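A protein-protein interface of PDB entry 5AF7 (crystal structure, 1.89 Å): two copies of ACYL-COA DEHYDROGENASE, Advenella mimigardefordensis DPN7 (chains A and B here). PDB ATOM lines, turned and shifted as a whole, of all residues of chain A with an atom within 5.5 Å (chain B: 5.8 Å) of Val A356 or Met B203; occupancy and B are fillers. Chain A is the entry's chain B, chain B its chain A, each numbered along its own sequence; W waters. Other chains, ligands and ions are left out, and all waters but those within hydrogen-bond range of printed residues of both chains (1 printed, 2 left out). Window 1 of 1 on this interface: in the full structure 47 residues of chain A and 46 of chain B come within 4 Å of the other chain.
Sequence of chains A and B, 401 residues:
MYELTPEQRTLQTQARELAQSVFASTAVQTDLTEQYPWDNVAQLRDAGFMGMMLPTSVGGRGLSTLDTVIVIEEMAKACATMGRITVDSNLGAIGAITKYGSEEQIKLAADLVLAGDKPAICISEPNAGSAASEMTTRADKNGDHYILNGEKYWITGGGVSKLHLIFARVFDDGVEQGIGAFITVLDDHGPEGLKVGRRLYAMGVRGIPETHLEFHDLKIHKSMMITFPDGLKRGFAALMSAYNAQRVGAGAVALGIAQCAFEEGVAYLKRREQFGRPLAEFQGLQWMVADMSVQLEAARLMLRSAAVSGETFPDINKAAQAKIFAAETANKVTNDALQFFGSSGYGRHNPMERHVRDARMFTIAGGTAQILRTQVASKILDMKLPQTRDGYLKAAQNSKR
Of the 11 printed residues of chain B, 10 touch a printed residue of chain A. Hydrophobic or aromatic side chains of chain B that line the printed part of chain A: Tyr B201, Ala B202, Met B203 and Val B356. Of the 19 printed residues of chain A, 8 touch a printed residue of chain B. Among the printed residues, no Asp or Glu carboxylate lies within 4 Å of a Lys or Arg side-chain nitrogen of the other chain.
The backbone carbonyl oxygen (O) of Asn A331 lies close to the side-chain amide oxygen (OD1) of Asn A335 (2.8 Å). The side-chain carboxylate of Asp B31 lies within salt-bridge range of the guanidinium group of Arg B357, at 3.0 Å. The guanidinium group (NE) of Arg B206 sits at hydrogen-bond distance from the backbone carbonyl oxygen (O) of Ala B202 (2.9 Å). O of Met B203 sits at hydrogen-bond distance from NH1 of Arg B357. The side-chain carboxylate (OE1) of Glu A353 is in salt-bridge range of the guanidinium group (NE) of Arg A357 (2.7 Å). The backbone carbonyl oxygen (O) of Met A203 is in hydrogen-bond range of the guanidinium group (NH1) of Arg A357 (3.1 Å).
Water W1 bridges the guanidinium group of Arg B360 and the backbone carbonyl oxygen of Asn A335.
Met A203 touches Val B356, and with the chains exchanged Val A356 touches Met B203.
Met A203 touches Val B356 (CE to CG1, 3.98 Å). NH2 of Arg B360 touches CD2 of Leu A338, at 3.7 Å. Tyr A346 touches Ala B202 (O to CA, 3.4 Å). Val B205 touches Tyr A346. Asp B358 touches Tyr A346 (O to OH, 3.6 Å). Tyr A346 touches Arg B360. Gly A347 touches Tyr B201 (CA to O, 3.5 Å). Arg A348 touches Met B203 (CG to N, 3.8 Å). Met B203 touches Glu A353. CG1 of Val A356 touches CE of Met B203 (3.9 Å).
The guanidinium group (NE) of Arg B206 lies close to the guanidinium group (NH1) of Arg A348, 3.3 Å away. O of Ala B202 sits at hydrogen-bond distance from NH1 of Arg A348 (2.8 Å). N of Arg A348 is in hydrogen-bond range of O of Tyr B201, at 2.8 Å. The backbone NH (N) of Gly B204 lies within hydrogen-bond range of the side-chain hydroxyl (OH) of Tyr A346 (3.1 Å). The side-chain hydroxyl (OH) of Tyr A346 is in hydrogen-bond range of the backbone carbonyl oxygen (O) of Arg B357. The backbone carbonyl oxygen (O) of Tyr A346 is in hydrogen-bond range of the backbone NH (N) of Met B203 (2.9 Å). The guanidinium group of Arg B360 lies within hydrogen-bond range of the backbone carbonyl oxygen of Asn A335 (2.8 Å).
Met B203 touches just these residues of chain A: Tyr A346 (2.9 Å), Arg A348 (3.8 Å), Glu A353 (3.6 Å) and Val A356 (3.9 Å). Of the printed residues of chain A, Arg B357 touches Tyr A346 (2.7 Å). Printed residues of chain B within 4 Å of Arg A348: Tyr B201 (2.8 Å), Ala B202 (2.8 Å), Met B203 (3.8 Å) and Arg B206 (3.3 Å). Ala A359 touches none of the printed residues of chain B. The nearest printed residue of chain A that does not touch Met B203 is Arg A357 (4.3 Å). The nearest printed residue of chain A that does not touch Arg B360 is Val A356 (5.5 Å).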
ATOM      1  N   MET A 203       5.708 -26.402  -1.551  1.00  0.00           N
ATOM      2  CA  MET A 203       6.565 -25.787  -2.552  1.00  0.00           C
ATOM      3  C   MET A 203       5.800 -25.502  -3.842  1.00  0.00           C
ATOM      4  O   MET A 203       5.928 -24.423  -4.420  1.00  0.00           O
ATOM      5  CB  MET A 203       7.763 -26.692  -2.846  1.00  0.00           C
ATOM      6  CG  MET A 203       8.716 -26.168  -3.892  1.00  0.00           C
ATOM      7  SD  MET A 203       9.992 -27.415  -4.167  1.00  0.00           S
ATOM      8  CE  MET A 203      11.335 -26.352  -4.675  1.00  0.00           C
ATOM      9  N   ILE A 257       3.571 -30.990 -17.102  1.00  0.00           N
ATOM     10  CA  ILE A 257       4.286 -29.827 -16.595  1.00  0.00           C
ATOM     11  C   ILE A 257       5.577 -29.610 -17.385  1.00  0.00           C
ATOM     12  O   ILE A 257       5.871 -28.498 -17.837  1.00  0.00           O
ATOM     13  CB  ILE A 257       4.617 -29.984 -15.091  1.00  0.00           C
ATOM     14  CG1 ILE A 257       3.332 -30.060 -14.263  1.00  0.00           C
ATOM     15  CG2 ILE A 257       5.474 -28.847 -14.604  1.00  0.00           C
ATOM     16  CD1 ILE A 257       3.565 -30.560 -12.825  1.00  0.00           C
ATOM     17  N   ASN A 331      11.828 -33.114 -13.570  1.00  0.00           N
ATOM     18  CA  ASN A 331      12.706 -32.254 -12.767  1.00  0.00           C
ATOM     19  C   ASN A 331      13.847 -31.695 -13.625  1.00  0.00           C
ATOM     20  O   ASN A 331      14.200 -30.515 -13.525  1.00  0.00           O
ATOM     21  CB  ASN A 331      13.261 -33.014 -11.556  1.00  0.00           C
ATOM     22  CG  ASN A 331      12.203 -33.249 -10.477  1.00  0.00           C
ATOM     23  OD1 ASN A 331      11.216 -32.519 -10.400  1.00  0.00           O
ATOM     24  ND2 ASN A 331      12.412 -34.267  -9.637  1.00  0.00           N
ATOM     25  N   THR A 334      12.170 -29.188 -16.573  1.00  0.00           N
ATOM     26  CA  THR A 334      11.675 -27.894 -16.085  1.00  0.00           C
ATOM     27  C   THR A 334      12.832 -26.989 -15.678  1.00  0.00           C
ATOM     28  O   THR A 334      12.784 -25.792 -15.918  1.00  0.00           O
ATOM     29  CB  THR A 334      10.691 -28.025 -14.901  1.00  0.00           C
ATOM     30  OG1 THR A 334      11.298 -28.726 -13.809  1.00  0.00           O
ATOM     31  CG2 THR A 334       9.410 -28.732 -15.333  1.00  0.00           C
ATOM     32  N   ASN A 335      13.878 -27.550 -15.079  1.00  0.00           N
ATOM     33  CA  ASN A 335      15.009 -26.728 -14.673  1.00  0.00           C
ATOM     34  C   ASN A 335      15.749 -26.187 -15.879  1.00  0.00           C
ATOM     35  O   ASN A 335      16.152 -25.022 -15.902  1.00  0.00           O
ATOM     36  CB  ASN A 335      15.980 -27.506 -13.781  1.00  0.00           C
ATOM     37  CG  ASN A 335      15.566 -27.478 -12.309  1.00  0.00           C
ATOM     38  OD1 ASN A 335      15.043 -28.459 -11.771  1.00  0.00           O
ATOM     39  ND2 ASN A 335      15.764 -26.339 -11.671  1.00  0.00           N
ATOM     40  N   LEU A 338      13.736 -23.496 -17.700  1.00  0.00           N
ATOM     41  CA  LEU A 338      13.924 -22.269 -16.925  1.00  0.00           C
ATOM     42  C   LEU A 338      15.234 -21.590 -17.310  1.00  0.00           C
ATOM     43  O   LEU A 338      15.303 -20.363 -17.426  1.00  0.00           O
ATOM     44  CB  LEU A 338      13.904 -22.568 -15.410  1.00  0.00           C
ATOM     45  CG  LEU A 338      13.876 -21.376 -14.445  1.00  0.00           C
ATOM     46  CD1 LEU A 338      13.268 -21.779 -13.104  1.00  0.00           C
ATOM     47  CD2 LEU A 338      15.270 -20.784 -14.228  1.00  0.00           C
ATOM     48  N   TYR A 346      13.960 -16.732 -13.450  1.00  0.00           N
ATOM     49  CA  TYR A 346      13.983 -16.730 -11.984  1.00  0.00           C
ATOM     50  C   TYR A 346      12.919 -15.796 -11.397  1.00  0.00           C
ATOM     51  O   TYR A 346      12.668 -15.800 -10.182  1.00  0.00           O
ATOM     52  CB  TYR A 346      15.372 -16.325 -11.491  1.00  0.00           C
ATOM     53  CG  TYR A 346      15.703 -16.734 -10.080  1.00  0.00           C
ATOM     54  CD1 TYR A 346      15.792 -18.078  -9.731  1.00  0.00           C
ATOM     55  CD2 TYR A 346      15.964 -15.777  -9.096  1.00  0.00           C
ATOM     56  CE1 TYR A 346      16.119 -18.462  -8.443  1.00  0.00           C
ATOM     57  CE2 TYR A 346      16.297 -16.156  -7.801  1.00  0.00           C
ATOM     58  CZ  TYR A 346      16.368 -17.507  -7.488  1.00  0.00           C
ATOM     59  OH  TYR A 346      16.700 -17.895  -6.210  1.00  0.00           O
ATOM     60  N   GLY A 347      12.290 -14.998 -12.258  1.00  0.00           N
ATOM     61  CA  GLY A 347      11.229 -14.097 -11.821  1.00  0.00           C
ATOM     62  C   GLY A 347       9.875 -14.779 -11.736  1.00  0.00           C
ATOM     63  O   GLY A 347       9.498 -15.542 -12.629  1.00  0.00           O
ATOM     64  N   ARG A 348       9.130 -14.511 -10.665  1.00  0.00           N
ATOM     65  CA  ARG A 348       7.836 -15.165 -10.485  1.00  0.00           C
ATOM     66  C   ARG A 348       6.770 -14.574 -11.410  1.00  0.00           C
ATOM     67  O   ARG A 348       5.647 -15.079 -11.462  1.00  0.00           O
ATOM     68  CB  ARG A 348       7.378 -15.075  -9.028  1.00  0.00           C
ATOM     69  CG  ARG A 348       8.460 -15.501  -8.036  1.00  0.00           C
ATOM     70  CD  ARG A 348       7.864 -16.043  -6.750  1.00  0.00           C
ATOM     71  NE  ARG A 348       7.028 -15.077  -6.034  1.00  0.00           N
ATOM     72  CZ  ARG A 348       7.449 -14.300  -5.040  1.00  0.00           C
ATOM     73  NH1 ARG A 348       8.717 -14.342  -4.638  1.00  0.00           N
ATOM     74  NH2 ARG A 348       6.593 -13.479  -4.436  1.00  0.00           N
ATOM     75  N   PRO A 351       6.220 -18.104 -15.638  1.00  0.00           N
ATOM     76  CA  PRO A 351       5.780 -19.378 -15.058  1.00  0.00           C
ATOM     77  C   PRO A 351       6.868 -20.451 -14.920  1.00  0.00           C
ATOM     78  O   PRO A 351       6.583 -21.544 -14.433  1.00  0.00           O
ATOM     79  CB  PRO A 351       4.718 -19.845 -16.057  1.00  0.00           C
ATOM     80  CG  PRO A 351       5.226 -19.356 -17.360  1.00  0.00           C
ATOM     81  CD  PRO A 351       5.832 -17.994 -17.060  1.00  0.00           C
ATOM     82  N   MET A 352       8.090 -20.159 -15.335  1.00  0.00           N
ATOM     83  CA  MET A 352       9.119 -21.207 -15.355  1.00  0.00           C
ATOM     84  C   MET A 352       9.523 -21.681 -13.961  1.00  0.00           C
ATOM     85  O   MET A 352       9.762 -22.875 -13.755  1.00  0.00           O
ATOM     86  CB  MET A 352      10.350 -20.714 -16.110  1.00  0.00           C
ATOM     87  CG  MET A 352      10.006 -20.124 -17.458  1.00  0.00           C
ATOM     88  SD  MET A 352       8.970 -21.183 -18.477  1.00  0.00           S
ATOM     89  CE  MET A 352      10.125 -22.473 -18.928  1.00  0.00           C
ATOM     90  N   GLU A 353       9.604 -20.765 -12.999  1.00  0.00           N
ATOM     91  CA  GLU A 353      10.007 -21.170 -11.659  1.00  0.00           C
ATOM     92  C   GLU A 353       8.885 -21.985 -11.015  1.00  0.00           C
ATOM     93  O   GLU A 353       9.144 -22.900 -10.243  1.00  0.00           O
ATOM     94  CB  GLU A 353      10.391 -19.958 -10.793  1.00  0.00           C
ATOM     95  CG  GLU A 353       9.297 -18.917 -10.603  1.00  0.00           C
ATOM     96  CD  GLU A 353       8.464 -19.161  -9.361  1.00  0.00           C
ATOM     97  OE1 GLU A 353       8.988 -19.790  -8.415  1.00  0.00           O
ATOM     98  OE2 GLU A 353       7.289 -18.708  -9.323  1.00  0.00           O
ATOM     99  N   ARG A 354       7.634 -21.668 -11.349  1.00  0.00           N
ATOM    100  CA  ARG A 354       6.525 -22.469 -10.855  1.00  0.00           C
ATOM    101  C   ARG A 354       6.599 -23.898 -11.404  1.00  0.00           C
ATOM    102  O   ARG A 354       6.282 -24.855 -10.695  1.00  0.00           O
ATOM    103  CB  ARG A 354       5.182 -21.833 -11.222  1.00  0.00           C
ATOM    104  CG  ARG A 354       3.974 -22.533 -10.603  1.00  0.00           C
ATOM    105  CD  ARG A 354       2.674 -22.079 -11.265  1.00  0.00           C
ATOM    106  NE  ARG A 354       2.392 -22.769 -12.520  1.00  0.00           N
ATOM    107  CZ  ARG A 354       2.094 -22.162 -13.671  1.00  0.00           C
ATOM    108  NH1 ARG A 354       2.067 -20.838 -13.755  1.00  0.00           N
ATOM    109  NH2 ARG A 354       1.831 -22.885 -14.745  1.00  0.00           N
ATOM    110  N   HIS A 355       7.014 -24.054 -12.660  1.00  0.00           N
ATOM    111  CA  HIS A 355       7.049 -25.403 -13.242  1.00  0.00           C
ATOM    112  C   HIS A 355       8.007 -26.289 -12.467  1.00  0.00           C
ATOM    113  O   HIS A 355       7.744 -27.468 -12.257  1.00  0.00           O
ATOM    114  CB  HIS A 355       7.452 -25.367 -14.713  1.00  0.00           C
ATOM    115  CG  HIS A 355       6.453 -24.679 -15.587  1.00  0.00           C
ATOM    116  ND1 HIS A 355       6.809 -23.980 -16.721  1.00  0.00           N
ATOM    117  CD2 HIS A 355       5.108 -24.569 -15.483  1.00  0.00           C
ATOM    118  CE1 HIS A 355       5.722 -23.477 -17.281  1.00  0.00           C
ATOM    119  NE2 HIS A 355       4.676 -23.826 -16.554  1.00  0.00           N
ATOM    120  N   VAL A 356       9.131 -25.714 -12.063  1.00  0.00           N
ATOM    121  CA  VAL A 356      10.118 -26.440 -11.272  1.00  0.00           C
ATOM    122  C   VAL A 356       9.529 -26.811  -9.917  1.00  0.00           C
ATOM    123  O   VAL A 356       9.664 -27.950  -9.462  1.00  0.00           O
ATOM    124  CB  VAL A 356      11.409 -25.596 -11.075  1.00  0.00           C
ATOM    125  CG1 VAL A 356      12.357 -26.250 -10.047  1.00  0.00           C
ATOM    126  CG2 VAL A 356      12.124 -25.386 -12.420  1.00  0.00           C
ATOM    127  N   ARG A 357       8.874 -25.849  -9.273  1.00  0.00           N
ATOM    128  CA  ARG A 357       8.267 -26.102  -7.975  1.00  0.00           C
ATOM    129  C   ARG A 357       7.181 -27.158  -8.101  1.00  0.00           C
ATOM    130  O   ARG A 357       7.096 -28.048  -7.258  1.00  0.00           O
ATOM    131  CB  ARG A 357       7.681 -24.816  -7.364  1.00  0.00           C
ATOM    132  CG  ARG A 357       8.711 -23.751  -7.039  1.00  0.00           C
ATOM    133  CD  ARG A 357       8.102 -22.544  -6.292  1.00  0.00           C
ATOM    134  NE  ARG A 357       7.395 -21.591  -7.153  1.00  0.00           N
ATOM    135  CZ  ARG A 357       6.071 -21.466  -7.227  1.00  0.00           C
ATOM    136  NH1 ARG A 357       5.275 -22.252  -6.500  1.00  0.00           N
ATOM    137  NH2 ARG A 357       5.540 -20.542  -8.025  1.00  0.00           N
ATOM    138  N   ASP A 358       6.344 -27.046  -9.135  1.00  0.00           N
ATOM    139  CA  ASP A 358       5.261 -28.006  -9.350  1.00  0.00           C
ATOM    140  C   ASP A 358       5.796 -29.421  -9.627  1.00  0.00           C
ATOM    141  O   ASP A 358       5.334 -30.407  -9.043  1.00  0.00           O
ATOM    142  CB  ASP A 358       4.364 -27.571 -10.520  1.00  0.00           C
ATOM    143  CG  ASP A 358       3.504 -26.351 -10.197  1.00  0.00           C
ATOM    144  OD1 ASP A 358       3.354 -25.997  -9.002  1.00  0.00           O
ATOM    145  OD2 ASP A 358       2.972 -25.758 -11.157  1.00  0.00           O
ATOM    146  N   ALA A 359       6.748 -29.517 -10.546  1.00  0.00           N
ATOM    147  CA  ALA A 359       7.277 -30.828 -10.944  1.00  0.00           C
ATOM    148  C   ALA A 359       7.914 -31.576  -9.765  1.00  0.00           C
ATOM    149  O   ALA A 359       7.883 -32.810  -9.707  1.00  0.00           O
ATOM    150  CB  ALA A 359       8.286 -30.670 -12.087  1.00  0.00           C
ATOM    151  N   ARG A 360       8.472 -30.840  -8.813  1.00  0.00           N
ATOM    152  CA  ARG A 360       9.358 -31.470  -7.815  1.00  0.00           C
ATOM    153  C   ARG A 360       8.652 -32.486  -6.895  1.00  0.00           C
ATOM    154  O   ARG A 360       9.303 -33.355  -6.324  1.00  0.00           O
ATOM    155  CB  ARG A 360      10.047 -30.377  -6.978  1.00  0.00           C
ATOM    156  CG  ARG A 360      11.065 -30.876  -5.917  1.00  0.00           C
ATOM    157  CD  ARG A 360      12.216 -31.635  -6.571  1.00  0.00           C
ATOM    158  NE  ARG A 360      13.154 -32.234  -5.610  1.00  0.00           N
ATOM    159  CZ  ARG A 360      12.961 -33.400  -4.994  1.00  0.00           C
ATOM    160  NH1 ARG A 360      11.831 -34.085  -5.180  1.00  0.00           N
ATOM    161  NH2 ARG A 360      13.889 -33.868  -4.171  1.00  0.00           N
ATOM    162  N   ASP B  31      12.853 -15.098   4.222  1.00  0.00           N
ATOM    163  CA  ASP B  31      12.313 -15.639   2.968  1.00  0.00           C
ATOM    164  C   ASP B  31      10.808 -15.420   2.862  1.00  0.00           C
ATOM    165  O   ASP B  31      10.283 -15.127   1.780  1.00  0.00           O
ATOM    166  CB  ASP B  31      12.629 -17.128   2.833  1.00  0.00           C
ATOM    167  CG  ASP B  31      11.855 -17.796   1.692  1.00  0.00           C
ATOM    168  OD1 ASP B  31      12.216 -17.579   0.511  1.00  0.00           O
ATOM    169  OD2 ASP B  31      10.886 -18.536   1.984  1.00  0.00           O
ATOM    170  N   TYR B 201       9.856  -9.881  -8.180  1.00  0.00           N
ATOM    171  CA  TYR B 201       9.740 -10.943  -7.198  1.00  0.00           C
ATOM    172  C   TYR B 201      10.379 -12.215  -7.725  1.00  0.00           C
ATOM    173  O   TYR B 201      10.180 -12.568  -8.880  1.00  0.00           O
ATOM    174  CB  TYR B 201       8.275 -11.169  -6.849  1.00  0.00           C
ATOM    175  CG  TYR B 201       7.723 -10.037  -6.012  1.00  0.00           C
ATOM    176  CD1 TYR B 201       7.880 -10.030  -4.635  1.00  0.00           C
ATOM    177  CD2 TYR B 201       7.059  -8.974  -6.602  1.00  0.00           C
ATOM    178  CE1 TYR B 201       7.374  -8.989  -3.861  1.00  0.00           C
ATOM    179  CE2 TYR B 201       6.557  -7.934  -5.841  1.00  0.00           C
ATOM    180  CZ  TYR B 201       6.718  -7.946  -4.474  1.00  0.00           C
ATOM    181  OH  TYR B 201       6.217  -6.906  -3.714  1.00  0.00           O
ATOM    182  N   ALA B 202      11.135 -12.901  -6.873  1.00  0.00           N
ATOM    183  CA  ALA B 202      11.984 -13.990  -7.344  1.00  0.00           C
ATOM    184  C   ALA B 202      11.678 -15.336  -6.717  1.00  0.00           C
ATOM    185  O   ALA B 202      11.071 -15.451  -5.638  1.00  0.00           O
ATOM    186  CB  ALA B 202      13.460 -13.645  -7.101  1.00  0.00           C
ATOM    187  N   MET B 203      12.140 -16.368  -7.408  1.00  0.00           N
ATOM    188  CA  MET B 203      11.989 -17.729  -6.940  1.00  0.00           C
ATOM    189  C   MET B 203      12.595 -17.906  -5.550  1.00  0.00           C
ATOM    190  O   MET B 203      11.974 -18.514  -4.666  1.00  0.00           O
ATOM    191  CB  MET B 203      12.646 -18.685  -7.941  1.00  0.00           C
ATOM    192  CG  MET B 203      12.488 -20.147  -7.601  1.00  0.00           C
ATOM    193  SD  MET B 203      13.378 -21.172  -8.812  1.00  0.00           S
ATOM    194  CE  MET B 203      12.682 -22.774  -8.407  1.00  0.00           C
ATOM    195  N   GLY B 204      13.801 -17.370  -5.362  1.00  0.00           N
ATOM    196  CA  GLY B 204      14.491 -17.492  -4.081  1.00  0.00           C
ATOM    197  C   GLY B 204      15.370 -16.300  -3.749  1.00  0.00           C
ATOM    198  O   GLY B 204      15.309 -15.267  -4.427  1.00  0.00           O
ATOM    199  N   VAL B 205      16.221 -16.473  -2.733  1.00  0.00           N
ATOM    200  CA  VAL B 205      16.983 -15.393  -2.101  1.00  0.00           C
ATOM    201  C   VAL B 205      16.100 -14.125  -2.002  1.00  0.00           C
ATOM    202  O   VAL B 205      16.466 -13.022  -2.420  1.00  0.00           O
ATOM    203  CB  VAL B 205      18.316 -15.120  -2.843  1.00  0.00           C
ATOM    204  CG1 VAL B 205      19.247 -14.315  -1.950  1.00  0.00           C
ATOM    205  CG2 VAL B 205      18.983 -16.443  -3.205  1.00  0.00           C
ATOM    206  N   ARG B 206      14.925 -14.306  -1.411  1.00  0.00           N
ATOM    207  CA  ARG B 206      13.875 -13.298  -1.497  1.00  0.00           C
ATOM    208  C   ARG B 206      14.071 -12.125  -0.551  1.00  0.00           C
ATOM    209  O   ARG B 206      13.405 -11.103  -0.686  1.00  0.00           O
ATOM    210  CB  ARG B 206      12.518 -13.944  -1.247  1.00  0.00           C
ATOM    211  CG  ARG B 206      12.206 -15.042  -2.253  1.00  0.00           C
ATOM    212  CD  ARG B 206      10.831 -15.631  -1.997  1.00  0.00           C
ATOM    213  NE  ARG B 206      10.476 -16.590  -3.029  1.00  0.00           N
ATOM    214  CZ  ARG B 206       9.389 -17.348  -2.990  1.00  0.00           C
ATOM    215  NH1 ARG B 206       8.555 -17.250  -1.957  1.00  0.00           N
ATOM    216  NH2 ARG B 206       9.138 -18.204  -3.975  1.00  0.00           N
ATOM    217  N   VAL B 356      16.390 -25.179  -2.275  1.00  0.00           N
ATOM    218  CA  VAL B 356      16.357 -25.435  -3.720  1.00  0.00           C
ATOM    219  C   VAL B 356      16.073 -24.135  -4.474  1.00  0.00           C
ATOM    220  O   VAL B 356      16.752 -23.825  -5.442  1.00  0.00           O
ATOM    221  CB  VAL B 356      15.315 -26.509  -4.099  1.00  0.00           C
ATOM    222  CG1 VAL B 356      15.197 -26.610  -5.619  1.00  0.00           C
ATOM    223  CG2 VAL B 356      15.723 -27.878  -3.503  1.00  0.00           C
ATOM    224  N   ARG B 357      15.093 -23.362  -4.001  1.00  0.00           N
ATOM    225  CA  ARG B 357      14.741 -22.092  -4.636  1.00  0.00           C
ATOM    226  C   ARG B 357      15.910 -21.106  -4.592  1.00  0.00           C
ATOM    227  O   ARG B 357      16.190 -20.420  -5.575  1.00  0.00           O
ATOM    228  CB  ARG B 357      13.510 -21.474  -3.964  1.00  0.00           C
ATOM    229  CG  ARG B 357      12.225 -22.298  -4.115  1.00  0.00           C
ATOM    230  CD  ARG B 357      10.998 -21.510  -3.613  1.00  0.00           C
ATOM    231  NE  ARG B 357      10.842 -21.554  -2.156  1.00  0.00           N
ATOM    232  CZ  ARG B 357      11.127 -20.554  -1.320  1.00  0.00           C
ATOM    233  NH1 ARG B 357      11.611 -19.395  -1.767  1.00  0.00           N
ATOM    234  NH2 ARG B 357      10.921 -20.714  -0.017  1.00  0.00           N
ATOM    235  N   ASP B 358      16.577 -21.035  -3.444  1.00  0.00           N
ATOM    236  CA  ASP B 358      17.712 -20.142  -3.255  1.00  0.00           C
ATOM    237  C   ASP B 358      18.874 -20.523  -4.172  1.00  0.00           C
ATOM    238  O   ASP B 358      19.479 -19.656  -4.805  1.00  0.00           O
ATOM    239  CB  ASP B 358      18.186 -20.157  -1.795  1.00  0.00           C
ATOM    240  CG  ASP B 358      17.202 -19.492  -0.836  1.00  0.00           C
ATOM    241  OD1 ASP B 358      16.314 -18.732  -1.300  1.00  0.00           O
ATOM    242  OD2 ASP B 358      17.342 -19.709   0.387  1.00  0.00           O
ATOM    243  N   ARG B 360      18.957 -22.023  -6.990  1.00  0.00           N
ATOM    244  CA  ARG B 360      18.721 -22.068  -8.430  1.00  0.00           C
ATOM    245  C   ARG B 360      19.253 -20.849  -9.214  1.00  0.00           C
ATOM    246  O   ARG B 360      19.558 -20.972 -10.402  1.00  0.00           O
ATOM    247  CB  ARG B 360      17.223 -22.246  -8.712  1.00  0.00           C
ATOM    248  CG  ARG B 360      16.878 -22.468 -10.180  1.00  0.00           C
ATOM    249  CD  ARG B 360      17.576 -23.718 -10.719  1.00  0.00           C
ATOM    250  NE  ARG B 360      17.409 -23.888 -12.166  1.00  0.00           N
ATOM    251  CZ  ARG B 360      18.077 -23.188 -13.082  1.00  0.00           C
ATOM    252  NH1 ARG B 360      18.956 -22.256 -12.701  1.00  0.00           N
ATOM    253  NH2 ARG B 360      17.851 -23.407 -14.377  1.00  0.00           N
HETATM  254  O   HOH W   1      19.066 -26.566 -14.900  1.00  0.00           O
